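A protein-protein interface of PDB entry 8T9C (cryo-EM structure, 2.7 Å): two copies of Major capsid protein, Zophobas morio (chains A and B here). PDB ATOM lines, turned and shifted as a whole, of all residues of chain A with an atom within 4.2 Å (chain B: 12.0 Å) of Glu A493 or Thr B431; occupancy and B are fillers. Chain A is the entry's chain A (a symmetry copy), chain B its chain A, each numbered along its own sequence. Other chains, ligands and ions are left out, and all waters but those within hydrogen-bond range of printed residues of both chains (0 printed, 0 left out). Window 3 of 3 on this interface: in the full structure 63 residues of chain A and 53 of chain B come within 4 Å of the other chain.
ND2 of Asn A433 lies within hydrogen-bond range of O of Thr B431 (2.8 Å). The backbone carbonyl oxygen (O) of Val A495 lies within hydrogen-bond range of the backbone NH (N) of Thr B431 (2.8 Å). The side-chain amide oxygen (OD1) of Asn B433 lies within hydrogen-bond range of the side-chain amide nitrogen (ND2) of Asn A433, 3.0 Å away.
Asn B433 touches its own counterpart, Asn A433. Of the 8 pairs that touch across the chains among the printed residues, 1 has its exchanged pair printed and touching as well.
Among the printed residues, merely in contact across the chains: Val A495 with Gly B430 (3.2 Å), Thr A436 with Gly B430 (3.2 Å), Glu A493 with Thr B431 (3.5 Å), Thr A494 with Thr B431 (3.5 Å) and Thr A436 with Thr B431 (3.99 Å).
Of the printed residues of chain B, Glu A493 touches Thr B431. Of the printed residues of chain A, Thr B431 touches Asn A433 (2.8 Å), Thr A436 (3.99 Å), Glu A493 (3.5 Å), Thr A494 (3.5 Å) and Val A495 (2.8 Å). Of the printed residues of chain B, Asn A433 touches Thr B431 (2.8 Å) and Asn B433 (3.0 Å). No residue of chain B comes within 4 Å of Glu A434. No residue of chain B comes within 4 Å of Glu A488. No residue of chain B comes within 4 Å of Glu A489. No residue of chain B comes within 4 Å of Val A492. Of chain B, only Gly B430 (3.2 Å) and Thr B431 (2.8 Å) come within 4 Å of Val A495. Of the printed residues of chain A, Asn B433 touches Asn A433 (3.0 Å). Printed residues of chain B within 4 Å of Thr A436: Gly B430 and Thr B431. Of the printed residues of chain A, Gly B430 touches Thr A436 (3.2 Å) and Val A495 (3.2 Å). Glu B493 touches none of the printed residues of chain A. The nearest printed residue of chain B that does not touch Thr A436 is Ala B429 (5.7 Å).
The guanidinium group of Arg B453 lies within hydrogen-bond range of the side-chain amide oxygen of Asn B433 (3.2 Å). The side-chain amino group (NZ) of Lys A432 sits at hydrogen-bond distance from the side-chain hydroxyl (OG1) of Thr A494, 3.1 Å away. OG1 of Thr A436 sits at hydrogen-bond distance from OE1 of Glu A488, 2.7 Å away. N of Glu A489 is in hydrogen-bond range of OE1 of Glu A493 (3.1 Å).
Of the 18 printed residues of chain B, 3 touch a printed residue of chain A.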
ATOM      1  N   LYS A 432      26.752  -2.070  26.863  1.00  0.00           N
ATOM      2  CA  LYS A 432      25.534  -1.418  26.410  1.00  0.00           C
ATOM      3  C   LYS A 432      25.704  -0.886  24.992  1.00  0.00           C
ATOM      4  O   LYS A 432      26.777  -0.405  24.617  1.00  0.00           O
ATOM      5  CB  LYS A 432      25.168  -0.276  27.363  1.00  0.00           C
ATOM      6  CG  LYS A 432      24.035   0.623  26.894  1.00  0.00           C
ATOM      7  CD  LYS A 432      22.682  -0.060  26.989  1.00  0.00           C
ATOM      8  CE  LYS A 432      21.562   0.902  26.629  1.00  0.00           C
ATOM      9  NZ  LYS A 432      20.229   0.244  26.666  1.00  0.00           N
ATOM     10  N   ASN A 433      24.640  -0.992  24.198  1.00  0.00           N
ATOM     11  CA  ASN A 433      24.598  -0.393  22.866  1.00  0.00           C
ATOM     12  C   ASN A 433      24.081   1.030  23.007  1.00  0.00           C
ATOM     13  O   ASN A 433      22.897   1.263  23.247  1.00  0.00           O
ATOM     14  CB  ASN A 433      23.717  -1.206  21.925  1.00  0.00           C
ATOM     15  CG  ASN A 433      24.268  -2.584  21.657  1.00  0.00           C
ATOM     16  OD1 ASN A 433      25.477  -2.775  21.583  1.00  0.00           O
ATOM     17  ND2 ASN A 433      23.379  -3.557  21.508  1.00  0.00           N
ATOM     18  N   GLU A 434      24.983   2.000  22.880  1.00  0.00           N
ATOM     19  CA  GLU A 434      24.574   3.396  22.864  1.00  0.00           C
ATOM     20  C   GLU A 434      24.381   3.931  21.453  1.00  0.00           C
ATOM     21  O   GLU A 434      23.887   5.051  21.294  1.00  0.00           O
ATOM     22  CB  GLU A 434      25.592   4.253  23.615  1.00  0.00           C
ATOM     23  CG  GLU A 434      25.955   3.711  24.986  1.00  0.00           C
ATOM     24  CD  GLU A 434      26.837   4.654  25.775  1.00  0.00           C
ATOM     25  OE1 GLU A 434      26.819   5.868  25.487  1.00  0.00           O
ATOM     26  OE2 GLU A 434      27.549   4.183  26.685  1.00  0.00           O
ATOM     27  N   THR A 436      22.559   3.000  17.728  1.00  0.00           N
ATOM     28  CA  THR A 436      21.560   2.122  17.146  1.00  0.00           C
ATOM     29  C   THR A 436      22.123   1.394  15.928  1.00  0.00           C
ATOM     30  O   THR A 436      23.159   1.760  15.370  1.00  0.00           O
ATOM     31  CB  THR A 436      20.313   2.911  16.756  1.00  0.00           C
ATOM     32  OG1 THR A 436      20.665   3.921  15.804  1.00  0.00           O
ATOM     33  CG2 THR A 436      19.702   3.566  17.980  1.00  0.00           C
ATOM     34  N   GLU A 488      18.634   9.200  16.610  1.00  0.00           N
ATOM     35  CA  GLU A 488      19.523   8.929  17.727  1.00  0.00           C
ATOM     36  C   GLU A 488      19.725  10.186  18.563  1.00  0.00           C
ATOM     37  O   GLU A 488      19.644  11.313  18.073  1.00  0.00           O
ATOM     38  CB  GLU A 488      20.872   8.408  17.226  1.00  0.00           C
ATOM     39  CG  GLU A 488      20.931   6.909  17.036  1.00  0.00           C
ATOM     40  CD  GLU A 488      22.340   6.412  16.785  1.00  0.00           C
ATOM     41  OE1 GLU A 488      22.588   5.861  15.693  1.00  0.00           O
ATOM     42  OE2 GLU A 488      23.199   6.578  17.677  1.00  0.00           O
ATOM     43  N   GLU A 489      19.990   9.977  19.849  1.00  0.00           N
ATOM     44  CA  GLU A 489      20.426  11.031  20.746  1.00  0.00           C
ATOM     45  C   GLU A 489      21.802  10.669  21.279  1.00  0.00           C
ATOM     46  O   GLU A 489      22.134   9.493  21.440  1.00  0.00           O
ATOM     47  CB  GLU A 489      19.449  11.244  21.909  1.00  0.00           C
ATOM     48  CG  GLU A 489      18.151  11.903  21.512  1.00  0.00           C
ATOM     49  CD  GLU A 489      17.161  11.974  22.657  1.00  0.00           C
ATOM     50  OE1 GLU A 489      17.343  11.247  23.653  1.00  0.00           O
ATOM     51  OE2 GLU A 489      16.197  12.763  22.557  1.00  0.00           O
ATOM     52  N   ASN A 491      23.744  10.065  23.927  1.00  0.00           N
ATOM     53  CA  ASN A 491      23.758   9.728  25.341  1.00  0.00           C
ATOM     54  C   ASN A 491      23.512   8.234  25.468  1.00  0.00           C
ATOM     55  O   ASN A 491      23.299   7.542  24.472  1.00  0.00           O
ATOM     56  CB  ASN A 491      22.706  10.514  26.138  1.00  0.00           C
ATOM     57  CG  ASN A 491      21.285  10.164  25.738  1.00  0.00           C
ATOM     58  OD1 ASN A 491      20.984   9.984  24.561  1.00  0.00           O
ATOM     59  ND2 ASN A 491      20.405  10.061  26.725  1.00  0.00           N
ATOM     60  N   VAL A 492      23.551   7.738  26.702  1.00  0.00           N
ATOM     61  CA  VAL A 492      23.189   6.350  26.969  1.00  0.00           C
ATOM     62  C   VAL A 492      21.686   6.227  26.741  1.00  0.00           C
ATOM     63  O   VAL A 492      20.885   6.717  27.540  1.00  0.00           O
ATOM     64  CB  VAL A 492      23.576   5.919  28.386  1.00  0.00           C
ATOM     65  CG1 VAL A 492      23.164   4.476  28.626  1.00  0.00           C
ATOM     66  CG2 VAL A 492      25.069   6.091  28.604  1.00  0.00           C
ATOM     67  N   GLU A 493      21.303   5.577  25.646  1.00  0.00           N
ATOM     68  CA  GLU A 493      19.917   5.562  25.210  1.00  0.00           C
ATOM     69  C   GLU A 493      19.475   4.136  24.922  1.00  0.00           C
ATOM     70  O   GLU A 493      20.269   3.289  24.510  1.00  0.00           O
ATOM     71  CB  GLU A 493      19.720   6.424  23.958  1.00  0.00           C
ATOM     72  CG  GLU A 493      20.535   5.960  22.763  1.00  0.00           C
ATOM     73  CD  GLU A 493      20.224   6.738  21.504  1.00  0.00           C
ATOM     74  OE1 GLU A 493      19.252   7.522  21.513  1.00  0.00           O
ATOM     75  OE2 GLU A 493      20.950   6.564  20.502  1.00  0.00           O
ATOM     76  N   THR A 494      18.191   3.886  25.154  1.00  0.00           N
ATOM     77  CA  THR A 494      17.544   2.649  24.750  1.00  0.00           C
ATOM     78  C   THR A 494      16.560   2.965  23.634  1.00  0.00           C
ATOM     79  O   THR A 494      15.636   3.763  23.823  1.00  0.00           O
ATOM     80  CB  THR A 494      16.822   1.992  25.927  1.00  0.00           C
ATOM     81  OG1 THR A 494      17.707   1.916  27.049  1.00  0.00           O
ATOM     82  CG2 THR A 494      16.367   0.591  25.556  1.00  0.00           C
ATOM     83  N   VAL A 495      16.764   2.348  22.477  1.00  0.00           N
ATOM     84  CA  VAL A 495      15.968   2.622  21.290  1.00  0.00           C
ATOM     85  C   VAL A 495      15.457   1.301  20.737  1.00  0.00           C
ATOM     86  O   VAL A 495      16.204   0.323  20.650  1.00  0.00           O
ATOM     87  CB  VAL A 495      16.785   3.387  20.227  1.00  0.00           C
ATOM     88  CG1 VAL A 495      16.041   3.438  18.906  1.00  0.00           C
ATOM     89  CG2 VAL A 495      17.111   4.785  20.717  1.00  0.00           C
ATOM     90  N   TYR B 427      15.072  -2.091   8.430  1.00  0.00           N
ATOM     91  CA  TYR B 427      14.322  -1.425   9.482  1.00  0.00           C
ATOM     92  C   TYR B 427      15.232  -1.275  10.689  1.00  0.00           C
ATOM     93  O   TYR B 427      16.211  -2.017  10.827  1.00  0.00           O
ATOM     94  CB  TYR B 427      13.048  -2.201   9.842  1.00  0.00           C
ATOM     95  CG  TYR B 427      13.201  -3.701   9.831  1.00  0.00           C
ATOM     96  CD1 TYR B 427      13.642  -4.380  10.955  1.00  0.00           C
ATOM     97  CD2 TYR B 427      12.900  -4.437   8.696  1.00  0.00           C
ATOM     98  CE1 TYR B 427      13.777  -5.750  10.949  1.00  0.00           C
ATOM     99  CE2 TYR B 427      13.035  -5.805   8.681  1.00  0.00           C
ATOM    100  CZ  TYR B 427      13.472  -6.457   9.810  1.00  0.00           C
ATOM    101  OH  TYR B 427      13.607  -7.825   9.799  1.00  0.00           O
ATOM    102  N   PRO B 428      14.951  -0.319  11.574  1.00  0.00           N
ATOM    103  CA  PRO B 428      15.871  -0.077  12.691  1.00  0.00           C
ATOM    104  C   PRO B 428      15.750  -1.160  13.751  1.00  0.00           C
ATOM    105  O   PRO B 428      14.650  -1.526  14.167  1.00  0.00           O
ATOM    106  CB  PRO B 428      15.426   1.288  13.226  1.00  0.00           C
ATOM    107  CG  PRO B 428      14.005   1.384  12.862  1.00  0.00           C
ATOM    108  CD  PRO B 428      13.821   0.628  11.581  1.00  0.00           C
ATOM    109  N   ALA B 429      16.900  -1.678  14.179  1.00  0.00           N
ATOM    110  CA  ALA B 429      16.938  -2.574  15.323  1.00  0.00           C
ATOM    111  C   ALA B 429      17.093  -1.820  16.634  1.00  0.00           C
ATOM    112  O   ALA B 429      17.013  -2.436  17.702  1.00  0.00           O
ATOM    113  CB  ALA B 429      18.075  -3.584  15.167  1.00  0.00           C
ATOM    114  N   GLY B 430      17.299  -0.506  16.574  1.00  0.00           N
ATOM    115  CA  GLY B 430      17.529   0.259  17.786  1.00  0.00           C
ATOM    116  C   GLY B 430      18.826  -0.159  18.450  1.00  0.00           C
ATOM    117  O   GLY B 430      19.814  -0.496  17.790  1.00  0.00           O
ATOM    118  N   THR B 431      18.824  -0.140  19.778  1.00  0.00           N
ATOM    119  CA  THR B 431      19.965  -0.600  20.553  1.00  0.00           C
ATOM    120  C   THR B 431      19.859  -2.070  20.935  1.00  0.00           C
ATOM    121  O   THR B 431      20.732  -2.581  21.641  1.00  0.00           O
ATOM    122  CB  THR B 431      20.127   0.263  21.808  1.00  0.00           C
ATOM    123  OG1 THR B 431      18.910   0.249  22.563  1.00  0.00           O
ATOM    124  CG2 THR B 431      20.457   1.692  21.417  1.00  0.00           C
ATOM    125  N   LYS B 432      18.815  -2.756  20.484  1.00  0.00           N
ATOM    126  CA  LYS B 432      18.662  -4.182  20.729  1.00  0.00           C
ATOM    127  C   LYS B 432      19.448  -4.990  19.704  1.00  0.00           C
ATOM    128  O   LYS B 432      19.528  -4.623  18.529  1.00  0.00           O
ATOM    129  CB  LYS B 432      17.180  -4.564  20.680  1.00  0.00           C
ATOM    130  CG  LYS B 432      16.893  -6.057  20.711  1.00  0.00           C
ATOM    131  CD  LYS B 432      17.134  -6.661  22.083  1.00  0.00           C
ATOM    132  CE  LYS B 432      16.725  -8.124  22.113  1.00  0.00           C
ATOM    133  NZ  LYS B 432      16.998  -8.753  23.430  1.00  0.00           N
ATOM    134  N   ASN B 433      20.045  -6.089  20.162  1.00  0.00           N
ATOM    135  CA  ASN B 433      20.707  -7.045  19.276  1.00  0.00           C
ATOM    136  C   ASN B 433      19.669  -8.060  18.824  1.00  0.00           C
ATOM    137  O   ASN B 433      19.240  -8.926  19.586  1.00  0.00           O
ATOM    138  CB  ASN B 433      21.873  -7.729  19.978  1.00  0.00           C
ATOM    139  CG  ASN B 433      22.985  -6.772  20.328  1.00  0.00           C
ATOM    140  OD1 ASN B 433      23.259  -5.830  19.591  1.00  0.00           O
ATOM    141  ND2 ASN B 433      23.635  -7.009  21.459  1.00  0.00           N
ATOM    142  N   GLU B 434      19.237  -7.942  17.571  1.00  0.00           N
ATOM    143  CA  GLU B 434      18.346  -8.939  16.996  1.00  0.00           C
ATOM    144  C   GLU B 434      19.096 -10.011  16.219  1.00  0.00           C
ATOM    145  O   GLU B 434      18.483 -11.002  15.809  1.00  0.00           O
ATOM    146  CB  GLU B 434      17.311  -8.267  16.095  1.00  0.00           C
ATOM    147  CG  GLU B 434      16.611  -7.086  16.746  1.00  0.00           C
ATOM    148  CD  GLU B 434      15.481  -6.538  15.901  1.00  0.00           C
ATOM    149  OE1 GLU B 434      14.948  -7.288  15.059  1.00  0.00           O
ATOM    150  OE2 GLU B 434      15.124  -5.355  16.080  1.00  0.00           O
ATOM    151  N   VAL B 435      20.398  -9.838  16.014  1.00  0.00           N
ATOM    152  CA  VAL B 435      21.248 -10.830  15.370  1.00  0.00           C
ATOM    153  C   VAL B 435      22.248 -11.323  16.405  1.00  0.00           C
ATOM    154  O   VAL B 435      22.830 -10.522  17.145  1.00  0.00           O
ATOM    155  CB  VAL B 435      21.959 -10.248  14.137  1.00  0.00           C
ATOM    156  CG1 VAL B 435      23.024 -11.204  13.627  1.00  0.00           C
ATOM    157  CG2 VAL B 435      20.946  -9.943  13.044  1.00  0.00           C
ATOM    158  N   THR B 436      22.426 -12.638  16.478  1.00  0.00           N
ATOM    159  CA  THR B 436      23.346 -13.207  17.448  1.00  0.00           C
ATOM    160  C   THR B 436      24.792 -13.010  17.003  1.00  0.00           C
ATOM    161  O   THR B 436      25.083 -12.700  15.845  1.00  0.00           O
ATOM    162  CB  THR B 436      23.057 -14.691  17.655  1.00  0.00           C
ATOM    163  OG1 THR B 436      23.197 -15.384  16.411  1.00  0.00           O
ATOM    164  CG2 THR B 436      21.646 -14.883  18.181  1.00  0.00           C
ATOM    165  N   ALA B 437      25.707 -13.192  17.949  1.00  0.00           N
ATOM    166  CA  ALA B 437      27.131 -13.029  17.706  1.00  0.00           C
ATOM    167  C   ALA B 437      27.890 -14.214  18.281  1.00  0.00           C
ATOM    168  O   ALA B 437      27.480 -14.795  19.290  1.00  0.00           O
ATOM    169  CB  ALA B 437      27.657 -11.728  18.316  1.00  0.00           C
ATOM    170  N   GLN B 451      34.115 -10.744  19.743  1.00  0.00           N
ATOM    171  CA  GLN B 451      32.699 -10.931  19.464  1.00  0.00           C
ATOM    172  C   GLN B 451      32.425 -10.477  18.038  1.00  0.00           C
ATOM    173  O   GLN B 451      32.716  -9.330  17.684  1.00  0.00           O
ATOM    174  CB  GLN B 451      31.833 -10.153  20.456  1.00  0.00           C
ATOM    175  CG  GLN B 451      30.354 -10.461  20.371  1.00  0.00           C
ATOM    176  CD  GLN B 451      29.538  -9.684  21.384  1.00  0.00           C
ATOM    177  OE1 GLN B 451      29.706  -9.850  22.591  1.00  0.00           O
ATOM    178  NE2 GLN B 451      28.648  -8.830  20.897  1.00  0.00           N
ATOM    179  N   ARG B 453      29.503 -10.158  15.192  1.00  0.00           N
ATOM    180  CA  ARG B 453      28.111 -10.175  14.778  1.00  0.00           C
ATOM    181  C   ARG B 453      27.996 -10.671  13.339  1.00  0.00           C
ATOM    182  O   ARG B 453      28.948 -10.614  12.557  1.00  0.00           O
ATOM    183  CB  ARG B 453      27.505  -8.775  14.914  1.00  0.00           C
ATOM    184  CG  ARG B 453      25.998  -8.685  14.744  1.00  0.00           C
ATOM    185  CD  ARG B 453      25.266  -8.895  16.053  1.00  0.00           C
ATOM    186  NE  ARG B 453      25.646  -7.916  17.062  1.00  0.00           N
ATOM    187  CZ  ARG B 453      25.685  -8.161  18.363  1.00  0.00           C
ATOM    188  NH1 ARG B 453      25.340  -9.339  18.855  1.00  0.00           N
ATOM    189  NH2 ARG B 453      26.080  -7.201  19.193  1.00  0.00           N
ATOM    190  N   ASN B 491      13.299 -12.344  13.959  1.00  0.00           N
ATOM    191  CA  ASN B 491      12.409 -11.499  14.739  1.00  0.00           C
ATOM    192  C   ASN B 491      13.221 -10.879  15.864  1.00  0.00           C
ATOM    193  O   ASN B 491      14.410 -11.164  16.016  1.00  0.00           O
ATOM    194  CB  ASN B 491      11.215 -12.280  15.307  1.00  0.00           C
ATOM    195  CG  ASN B 491      11.628 -13.332  16.319  1.00  0.00           C
ATOM    196  OD1 ASN B 491      12.632 -14.019  16.145  1.00  0.00           O
ATOM    197  ND2 ASN B 491      10.854 -13.458  17.388  1.00  0.00           N
ATOM    198  N   VAL B 492      12.572 -10.023  16.649  1.00  0.00           N
ATOM    199  CA  VAL B 492      13.200  -9.474  17.847  1.00  0.00           C
ATOM    200  C   VAL B 492      13.332 -10.617  18.847  1.00  0.00           C
ATOM    201  O   VAL B 492      12.340 -11.067  19.426  1.00  0.00           O
ATOM    202  CB  VAL B 492      12.397  -8.310  18.432  1.00  0.00           C
ATOM    203  CG1 VAL B 492      13.076  -7.783  19.684  1.00  0.00           C
ATOM    204  CG2 VAL B 492      12.241  -7.203  17.403  1.00  0.00           C
ATOM    205  N   GLU B 493      14.558 -11.091  19.048  1.00  0.00           N
ATOM    206  CA  GLU B 493      14.795 -12.300  19.818  1.00  0.00           C
ATOM    207  C   GLU B 493      15.870 -12.054  20.863  1.00  0.00           C
ATOM    208  O   GLU B 493      16.783 -11.249  20.667  1.00  0.00           O
ATOM    209  CB  GLU B 493      15.217 -13.463  18.911  1.00  0.00           C
ATOM    210  CG  GLU B 493      16.501 -13.203  18.145  1.00  0.00           C
ATOM    211  CD  GLU B 493      16.971 -14.409  17.363  1.00  0.00           C
ATOM    212  OE1 GLU B 493      16.397 -15.502  17.551  1.00  0.00           O
ATOM    213  OE2 GLU B 493      17.918 -14.266  16.560  1.00  0.00           O
ATOM    214  N   THR B 494      15.742 -12.757  21.983  1.00  0.00           N
ATOM    215  CA  THR B 494      16.774 -12.806  23.005  1.00  0.00           C
ATOM    216  C   THR B 494      17.366 -14.208  23.020  1.00  0.00           C
ATOM    217  O   THR B 494      16.647 -15.188  23.242  1.00  0.00           O
ATOM    218  CB  THR B 494      16.209 -12.452  24.381  1.00  0.00           C
ATOM    219  OG1 THR B 494      15.454 -11.239  24.290  1.00  0.00           O
ATOM    220  CG2 THR B 494      17.333 -12.265  25.386  1.00  0.00           C
ATOM    221  N   VAL B 495      18.667 -14.300  22.775  1.00  0.00           N
ATOM    222  CA  VAL B 495      19.356 -15.577  22.659  1.00  0.00           C
ATOM    223  C   VAL B 495      20.567 -15.556  23.578  1.00  0.00           C
ATOM    224  O   VAL B 495      21.305 -14.567  23.627  1.00  0.00           O
ATOM    225  CB  VAL B 495      19.773 -15.861  21.200  1.00  0.00           C
ATOM    226  CG1 VAL B 495      20.710 -17.052  21.128  1.00  0.00           C
ATOM    227  CG2 VAL B 495      18.547 -16.084  20.335  1.00  0.00           C
